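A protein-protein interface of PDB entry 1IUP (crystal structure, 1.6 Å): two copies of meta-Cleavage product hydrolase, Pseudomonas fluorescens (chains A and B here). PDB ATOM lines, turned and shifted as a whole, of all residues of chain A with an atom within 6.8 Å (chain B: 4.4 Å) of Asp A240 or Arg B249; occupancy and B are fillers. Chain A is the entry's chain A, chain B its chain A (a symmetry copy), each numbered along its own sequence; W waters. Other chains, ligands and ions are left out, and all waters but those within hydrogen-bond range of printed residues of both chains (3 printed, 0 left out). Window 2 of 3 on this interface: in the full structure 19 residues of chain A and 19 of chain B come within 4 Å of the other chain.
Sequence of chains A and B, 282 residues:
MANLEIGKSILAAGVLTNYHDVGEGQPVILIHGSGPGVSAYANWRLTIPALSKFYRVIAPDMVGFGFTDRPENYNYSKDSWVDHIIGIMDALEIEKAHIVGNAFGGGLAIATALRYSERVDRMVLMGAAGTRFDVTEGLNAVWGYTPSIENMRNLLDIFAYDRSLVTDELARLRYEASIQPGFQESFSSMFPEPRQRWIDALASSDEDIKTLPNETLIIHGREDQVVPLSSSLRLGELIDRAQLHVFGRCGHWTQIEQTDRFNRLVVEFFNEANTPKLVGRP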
ATOM      1  N   ILE A 209      10.194 -18.277 -20.903  1.00  0.00           N
ATOM      2  CA  ILE A 209      10.773 -16.958 -20.696  1.00  0.00           C
ATOM      3  C   ILE A 209      11.563 -16.500 -21.920  1.00  0.00           C
ATOM      4  O   ILE A 209      11.570 -15.317 -22.248  1.00  0.00           O
ATOM      5  CB  ILE A 209      11.673 -16.949 -19.442  1.00  0.00           C
ATOM      6  CG1 ILE A 209      10.806 -17.176 -18.200  1.00  0.00           C
ATOM      7  CG2 ILE A 209      12.430 -15.627 -19.336  1.00  0.00           C
ATOM      8  CD1 ILE A 209      11.590 -17.308 -16.913  1.00  0.00           C
ATOM      9  N   LYS A 210      12.212 -17.439 -22.602  1.00  0.00           N
ATOM     10  CA  LYS A 210      12.989 -17.102 -23.792  1.00  0.00           C
ATOM     11  C   LYS A 210      12.116 -16.591 -24.936  1.00  0.00           C
ATOM     12  O   LYS A 210      12.620 -15.946 -25.855  1.00  0.00           O
ATOM     13  CB  LYS A 210      13.779 -18.319 -24.279  1.00  0.00           C
ATOM     14  CG  LYS A 210      14.946 -18.720 -23.397  1.00  0.00           C
ATOM     15  CD  LYS A 210      15.579 -20.002 -23.921  1.00  0.00           C
ATOM     16  CE  LYS A 210      16.738 -20.448 -23.055  1.00  0.00           C
ATOM     17  NZ  LYS A 210      17.278 -21.763 -23.507  1.00  0.00           N
ATOM     18  N   LEU A 212       9.652 -14.411 -24.597  1.00  0.00           N
ATOM     19  CA  LEU A 212       9.179 -13.056 -24.323  1.00  0.00           C
ATOM     20  C   LEU A 212       9.766 -12.050 -25.308  1.00  0.00           C
ATOM     21  O   LEU A 212      10.981 -11.924 -25.431  1.00  0.00           O
ATOM     22  CB  LEU A 212       9.537 -12.647 -22.891  1.00  0.00           C
ATOM     23  CG  LEU A 212       8.761 -13.353 -21.775  1.00  0.00           C
ATOM     24  CD1 LEU A 212       9.395 -13.026 -20.434  1.00  0.00           C
ATOM     25  CD2 LEU A 212       7.299 -12.921 -21.805  1.00  0.00           C
ATOM     26  N   PRO A 213       8.900 -11.320 -26.026  1.00  0.00           N
ATOM     27  CA  PRO A 213       9.354 -10.328 -27.003  1.00  0.00           C
ATOM     28  C   PRO A 213       9.489  -8.921 -26.427  1.00  0.00           C
ATOM     29  O   PRO A 213      10.058  -8.036 -27.062  1.00  0.00           O
ATOM     30  CB  PRO A 213       8.263 -10.393 -28.063  1.00  0.00           C
ATOM     31  CG  PRO A 213       7.032 -10.539 -27.213  1.00  0.00           C
ATOM     32  CD  PRO A 213       7.456 -11.584 -26.182  1.00  0.00           C
ATOM     33  N   ASN A 214       8.977  -8.736 -25.214  1.00  0.00           N
ATOM     34  CA  ASN A 214       8.967  -7.434 -24.542  1.00  0.00           C
ATOM     35  C   ASN A 214      10.300  -6.814 -24.146  1.00  0.00           C
ATOM     36  O   ASN A 214      11.202  -7.509 -23.682  1.00  0.00           O
ATOM     37  CB  ASN A 214       8.127  -7.510 -23.260  1.00  0.00           C
ATOM     38  CG  ASN A 214       6.913  -8.402 -23.397  1.00  0.00           C
ATOM     39  OD1 ASN A 214       7.034  -9.622 -23.519  1.00  0.00           O
ATOM     40  ND2 ASN A 214       5.730  -7.798 -23.369  1.00  0.00           N
ATOM     41  N   GLU A 215      10.413  -5.497 -24.328  1.00  0.00           N
ATOM     42  CA  GLU A 215      11.602  -4.772 -23.885  1.00  0.00           C
ATOM     43  C   GLU A 215      11.458  -4.921 -22.374  1.00  0.00           C
ATOM     44  O   GLU A 215      10.389  -4.634 -21.819  1.00  0.00           O
ATOM     45  CB  GLU A 215      11.525  -3.287 -24.257  1.00  0.00           C
ATOM     46  CG  GLU A 215      11.968  -2.932 -25.677  1.00  0.00           C
ATOM     47  CD  GLU A 215      13.471  -3.044 -25.881  1.00  0.00           C
ATOM     48  OE1 GLU A 215      14.231  -2.814 -24.916  1.00  0.00           O
ATOM     49  OE2 GLU A 215      13.899  -3.344 -27.014  1.00  0.00           O
ATOM     50  N   LEU A 235      17.534 -14.312 -15.369  1.00  0.00           N
ATOM     51  CA  LEU A 235      16.518 -13.670 -16.196  1.00  0.00           C
ATOM     52  C   LEU A 235      17.210 -12.842 -17.276  1.00  0.00           C
ATOM     53  O   LEU A 235      16.725 -12.740 -18.404  1.00  0.00           O
ATOM     54  CB  LEU A 235      15.618 -12.768 -15.342  1.00  0.00           C
ATOM     55  CG  LEU A 235      14.690 -13.466 -14.344  1.00  0.00           C
ATOM     56  CD1 LEU A 235      13.951 -12.417 -13.522  1.00  0.00           C
ATOM     57  CD2 LEU A 235      13.697 -14.354 -15.086  1.00  0.00           C
ATOM     58  N   GLY A 236      18.359 -12.268 -16.926  1.00  0.00           N
ATOM     59  CA  GLY A 236      19.112 -11.453 -17.864  1.00  0.00           C
ATOM     60  C   GLY A 236      19.701 -12.245 -19.017  1.00  0.00           C
ATOM     61  O   GLY A 236      20.001 -11.681 -20.068  1.00  0.00           O
ATOM     62  N   GLU A 237      19.874 -13.549 -18.822  1.00  0.00           N
ATOM     63  CA  GLU A 237      20.418 -14.408 -19.872  1.00  0.00           C
ATOM     64  C   GLU A 237      19.281 -14.944 -20.741  1.00  0.00           C
ATOM     65  O   GLU A 237      19.462 -15.191 -21.933  1.00  0.00           O
ATOM     66  CB  GLU A 237      21.162 -15.609 -19.275  1.00  0.00           C
ATOM     67  CG  GLU A 237      22.244 -15.288 -18.257  1.00  0.00           C
ATOM     68  CD  GLU A 237      22.962 -16.538 -17.756  1.00  0.00           C
ATOM     69  OE1 GLU A 237      22.284 -17.487 -17.296  1.00  0.00           O
ATOM     70  OE2 GLU A 237      24.210 -16.573 -17.821  1.00  0.00           O
ATOM     71  N   LEU A 238      18.110 -15.121 -20.132  1.00  0.00           N
ATOM     72  CA  LEU A 238      16.942 -15.672 -20.821  1.00  0.00           C
ATOM     73  C   LEU A 238      16.129 -14.706 -21.684  1.00  0.00           C
ATOM     74  O   LEU A 238      15.720 -15.054 -22.794  1.00  0.00           O
ATOM     75  CB  LEU A 238      16.014 -16.332 -19.794  1.00  0.00           C
ATOM     76  CG  LEU A 238      16.588 -17.514 -19.005  1.00  0.00           C
ATOM     77  CD1 LEU A 238      15.634 -17.897 -17.882  1.00  0.00           C
ATOM     78  CD2 LEU A 238      16.818 -18.696 -19.938  1.00  0.00           C
ATOM     79  N   ILE A 239      15.882 -13.504 -21.177  1.00  0.00           N
ATOM     80  CA  ILE A 239      15.091 -12.528 -21.918  1.00  0.00           C
ATOM     81  C   ILE A 239      15.952 -11.804 -22.947  1.00  0.00           C
ATOM     82  O   ILE A 239      16.970 -11.200 -22.607  1.00  0.00           O
ATOM     83  CB  ILE A 239      14.436 -11.527 -20.945  1.00  0.00           C
ATOM     84  CG1 ILE A 239      13.539 -12.297 -19.970  1.00  0.00           C
ATOM     85  CG2 ILE A 239      13.614 -10.497 -21.712  1.00  0.00           C
ATOM     86  CD1 ILE A 239      12.920 -11.441 -18.876  1.00  0.00           C
ATOM     87  N   ASP A 240      15.531 -11.853 -24.208  1.00  0.00           N
ATOM     88  CA  ASP A 240      16.307 -11.237 -25.280  1.00  0.00           C
ATOM     89  C   ASP A 240      16.478  -9.724 -25.212  1.00  0.00           C
ATOM     90  O   ASP A 240      17.606  -9.230 -25.146  1.00  0.00           O
ATOM     91  CB  ASP A 240      15.730 -11.619 -26.645  1.00  0.00           C
ATOM     92  CG  ASP A 240      16.615 -11.167 -27.790  1.00  0.00           C
ATOM     93  OD1 ASP A 240      17.816 -11.513 -27.783  1.00  0.00           O
ATOM     94  OD2 ASP A 240      16.114 -10.470 -28.692  1.00  0.00           O
ATOM     95  N   ARG A 241      15.375  -8.983 -25.254  1.00  0.00           N
ATOM     96  CA  ARG A 241      15.449  -7.525 -25.204  1.00  0.00           C
ATOM     97  C   ARG A 241      15.479  -7.066 -23.760  1.00  0.00           C
ATOM     98  O   ARG A 241      14.590  -6.352 -23.303  1.00  0.00           O
ATOM     99  CB  ARG A 241      14.248  -6.906 -25.920  1.00  0.00           C
ATOM    100  CG  ARG A 241      14.251  -7.137 -27.419  1.00  0.00           C
ATOM    101  CD  ARG A 241      13.051  -6.482 -28.079  1.00  0.00           C
ATOM    102  NE  ARG A 241      13.145  -6.527 -29.535  1.00  0.00           N
ATOM    103  CZ  ARG A 241      14.025  -5.831 -30.250  1.00  0.00           C
ATOM    104  NH1 ARG A 241      14.890  -5.028 -29.645  1.00  0.00           N
ATOM    105  NH2 ARG A 241      14.042  -5.942 -31.572  1.00  0.00           N
ATOM    106  N   ALA A 242      16.525  -7.464 -23.048  1.00  0.00           N
ATOM    107  CA  ALA A 242      16.637  -7.118 -21.646  1.00  0.00           C
ATOM    108  C   ALA A 242      17.846  -6.286 -21.266  1.00  0.00           C
ATOM    109  O   ALA A 242      18.879  -6.308 -21.932  1.00  0.00           O
ATOM    110  CB  ALA A 242      16.628  -8.392 -20.809  1.00  0.00           C
ATOM    111  N   GLN A 243      17.676  -5.538 -20.185  1.00  0.00           N
ATOM    112  CA  GLN A 243      18.735  -4.733 -19.602  1.00  0.00           C
ATOM    113  C   GLN A 243      18.718  -5.150 -18.145  1.00  0.00           C
ATOM    114  O   GLN A 243      17.652  -5.418 -17.581  1.00  0.00           O
ATOM    115  CB  GLN A 243      18.435  -3.238 -19.685  1.00  0.00           C
ATOM    116  CG  GLN A 243      18.513  -2.641 -21.070  1.00  0.00           C
ATOM    117  CD  GLN A 243      18.172  -1.171 -21.058  1.00  0.00           C
ATOM    118  OE1 GLN A 243      18.990  -0.328 -20.672  1.00  0.00           O
ATOM    119  NE2 GLN A 243      16.949  -0.849 -21.461  1.00  0.00           N
ATOM    120  N   TYR B 161      27.169  -6.296 -32.152  1.00  0.00           N
ATOM    121  CA  TYR B 161      26.143  -7.287 -31.896  1.00  0.00           C
ATOM    122  C   TYR B 161      25.397  -7.386 -33.226  1.00  0.00           C
ATOM    123  O   TYR B 161      25.180  -8.474 -33.756  1.00  0.00           O
ATOM    124  CB  TYR B 161      25.178  -6.817 -30.809  1.00  0.00           C
ATOM    125  CG  TYR B 161      23.901  -7.618 -30.788  1.00  0.00           C
ATOM    126  CD1 TYR B 161      23.879  -8.921 -30.298  1.00  0.00           C
ATOM    127  CD2 TYR B 161      22.725  -7.092 -31.321  1.00  0.00           C
ATOM    128  CE1 TYR B 161      22.710  -9.687 -30.341  1.00  0.00           C
ATOM    129  CE2 TYR B 161      21.556  -7.845 -31.368  1.00  0.00           C
ATOM    130  CZ  TYR B 161      21.556  -9.138 -30.879  1.00  0.00           C
ATOM    131  OH  TYR B 161      20.395  -9.880 -30.931  1.00  0.00           O
ATOM    132  N   ARG B 222      25.977  -7.634 -22.956  1.00  0.00           N
ATOM    133  CA  ARG B 222      25.824  -9.059 -22.691  1.00  0.00           C
ATOM    134  C   ARG B 222      26.609  -9.953 -23.645  1.00  0.00           C
ATOM    135  O   ARG B 222      27.270 -10.905 -23.220  1.00  0.00           O
ATOM    136  CB  ARG B 222      24.340  -9.445 -22.736  1.00  0.00           C
ATOM    137  CG  ARG B 222      24.068 -10.918 -22.467  1.00  0.00           C
ATOM    138  CD  ARG B 222      22.575 -11.193 -22.414  1.00  0.00           C
ATOM    139  NE  ARG B 222      21.926 -10.918 -23.695  1.00  0.00           N
ATOM    140  CZ  ARG B 222      20.614 -10.762 -23.854  1.00  0.00           C
ATOM    141  NH1 ARG B 222      19.799 -10.848 -22.810  1.00  0.00           N
ATOM    142  NH2 ARG B 222      20.117 -10.524 -25.060  1.00  0.00           N
ATOM    143  N   GLU B 223      26.542  -9.629 -24.931  1.00  0.00           N
ATOM    144  CA  GLU B 223      27.204 -10.415 -25.963  1.00  0.00           C
ATOM    145  C   GLU B 223      28.667 -10.056 -26.260  1.00  0.00           C
ATOM    146  O   GLU B 223      29.227 -10.519 -27.255  1.00  0.00           O
ATOM    147  CB  GLU B 223      26.386 -10.336 -27.259  1.00  0.00           C
ATOM    148  CG  GLU B 223      25.015 -11.039 -27.224  1.00  0.00           C
ATOM    149  CD  GLU B 223      23.911 -10.233 -26.544  1.00  0.00           C
ATOM    150  OE1 GLU B 223      24.124  -9.048 -26.220  1.00  0.00           O
ATOM    151  OE2 GLU B 223      22.812 -10.794 -26.348  1.00  0.00           O
ATOM    152  N   PHE B 247      23.649  -4.339 -20.964  1.00  0.00           N
ATOM    153  CA  PHE B 247      22.771  -4.169 -22.115  1.00  0.00           C
ATOM    154  C   PHE B 247      22.680  -5.466 -22.905  1.00  0.00           C
ATOM    155  O   PHE B 247      23.700  -5.985 -23.363  1.00  0.00           O
ATOM    156  CB  PHE B 247      23.315  -3.105 -23.077  1.00  0.00           C
ATOM    157  CG  PHE B 247      23.287  -1.703 -22.543  1.00  0.00           C
ATOM    158  CD1 PHE B 247      22.079  -1.059 -22.283  1.00  0.00           C
ATOM    159  CD2 PHE B 247      24.473  -1.001 -22.363  1.00  0.00           C
ATOM    160  CE1 PHE B 247      22.057   0.269 -21.854  1.00  0.00           C
ATOM    161  CE2 PHE B 247      24.463   0.324 -21.937  1.00  0.00           C
ATOM    162  CZ  PHE B 247      23.254   0.962 -21.682  1.00  0.00           C
ATOM    163  N   GLY B 248      21.468  -5.993 -23.058  1.00  0.00           N
ATOM    164  CA  GLY B 248      21.295  -7.188 -23.866  1.00  0.00           C
ATOM    165  C   GLY B 248      21.332  -6.712 -25.310  1.00  0.00           C
ATOM    166  O   GLY B 248      21.102  -5.526 -25.569  1.00  0.00           O
ATOM    167  N   ARG B 249      21.619  -7.617 -26.245  1.00  0.00           N
ATOM    168  CA  ARG B 249      21.700  -7.269 -27.667  1.00  0.00           C
ATOM    169  C   ARG B 249      22.720  -6.148 -27.851  1.00  0.00           C
ATOM    170  O   ARG B 249      22.464  -5.143 -28.515  1.00  0.00           O
ATOM    171  CB  ARG B 249      20.326  -6.834 -28.192  1.00  0.00           C
ATOM    172  CG  ARG B 249      19.275  -7.942 -28.151  1.00  0.00           C
ATOM    173  CD  ARG B 249      17.892  -7.414 -28.513  1.00  0.00           C
ATOM    174  NE  ARG B 249      17.804  -6.994 -29.908  1.00  0.00           N
ATOM    175  CZ  ARG B 249      17.509  -7.804 -30.921  1.00  0.00           C
ATOM    176  NH1 ARG B 249      17.263  -9.090 -30.704  1.00  0.00           N
ATOM    177  NH2 ARG B 249      17.464  -7.326 -32.157  1.00  0.00           N
ATOM    178  N   CYS B 250      23.890  -6.342 -27.257  1.00  0.00           N
ATOM    179  CA  CYS B 250      24.944  -5.346 -27.325  1.00  0.00           C
ATOM    180  C   CYS B 250      26.291  -6.019 -27.114  1.00  0.00           C
ATOM    181  O   CYS B 250      26.445  -6.851 -26.222  1.00  0.00           O
ATOM    182  CB  CYS B 250      24.703  -4.284 -26.247  1.00  0.00           C
ATOM    183  SG  CYS B 250      25.883  -2.918 -26.205  1.00  0.00           S
HETATM  184  O   HOH W   1      19.943 -11.741 -29.277  1.00  0.00           O
HETATM  185  O   HOH W   2      20.717 -13.886 -24.105  1.00  0.00           O
HETATM  186  O   HOH W   3      18.195  -4.367 -29.873  1.00  0.00           O
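OE2 of Glu A215 lies within salt-bridge range of NH1 of Arg A241 (3.3 Å).
The side-chain hydroxyl of Tyr B161 lies within hydrogen-bond range of the guanidinium group of Arg B249 (3.2 Å).
NE of Arg B222 is in salt-bridge range of OE2 of Glu B223 (2.8 Å).
The backbone carbonyl oxygen of Phe B247 sits at hydrogen-bond distance from the backbone NH of Arg B222 (2.8 Å).
N of Arg B222 is in hydrogen-bond range of O of Cys B250, at 3.4 Å.
The side-chain carboxylate (OE1) of Glu B223 is in hydrogen-bond range of the backbone NH (N) of Arg B249 (2.9 Å).
No position is printed for both chains.
Of the 7 pairs that touch across the chains among the printed residues, none has its exchanged pair printed and touching as well.
Among the printed residues, 7 pairs touch across the chains.
Among the printed residues, merely in contact across the chains: Gln A243 with Phe B247 and Arg A241 with Arg B249.
The backbone carbonyl oxygen of Gly A236 is in hydrogen-bond range of the guanidinium group of Arg B222, 2.9 Å away.
The backbone carbonyl oxygen (O) of Ile A239 is in hydrogen-bond range of the guanidinium group (NH1) of Arg B222 (2.9 Å).
OD1 of Asp A240 is in salt-bridge range of NH2 of Arg B222, 3.7 Å away.
The side-chain carboxylate (OD2) of Asp A240 is in salt-bridge range of the guanidinium group (NH1) of Arg B249, at 2.7 Å.
The backbone carbonyl oxygen (O) of Ala A242 is in hydrogen-bond range of the backbone NH (N) of Gly B248.
Water W1 lies within hydrogen-bond range of OH of Tyr B161 (2.5 Å) and OD1 of Asp A240 (2.6 Å).
Water W3 bridges the guanidinium group of Arg B249 and the guanidinium group of Arg A241.
Water W2 lies within hydrogen-bond range of the backbone carbonyl oxygen of Glu A237 (2.8 Å) and the guanidinium group of Arg B222 (3.2 Å).
Asn A214 touches none of the printed residues of chain B.
Of chain B, only Arg B222 (2.8 Å) and Arg B249 (2.7 Å) come within 4 Å of Asp A240.
Of the printed residues of chain B, Ala A242 touches Gly B248.
Printed residues of chain B within 4 Å of Gln A243: Phe B247 (3.3 Å).
Of the printed residues of chain A, Arg B222 touches Gly A236 (2.9 Å), Ile A239 (2.9 Å) and Asp A240 (2.8 Å).
Arg B249 touches two residues of chain A.
The nearest residue of chain A that does not touch Arg B249 is Ala A242 (5.3 Å).
The nearest printed residue of chain B that does not touch Ala A242 is Phe B247 (4.01 Å).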
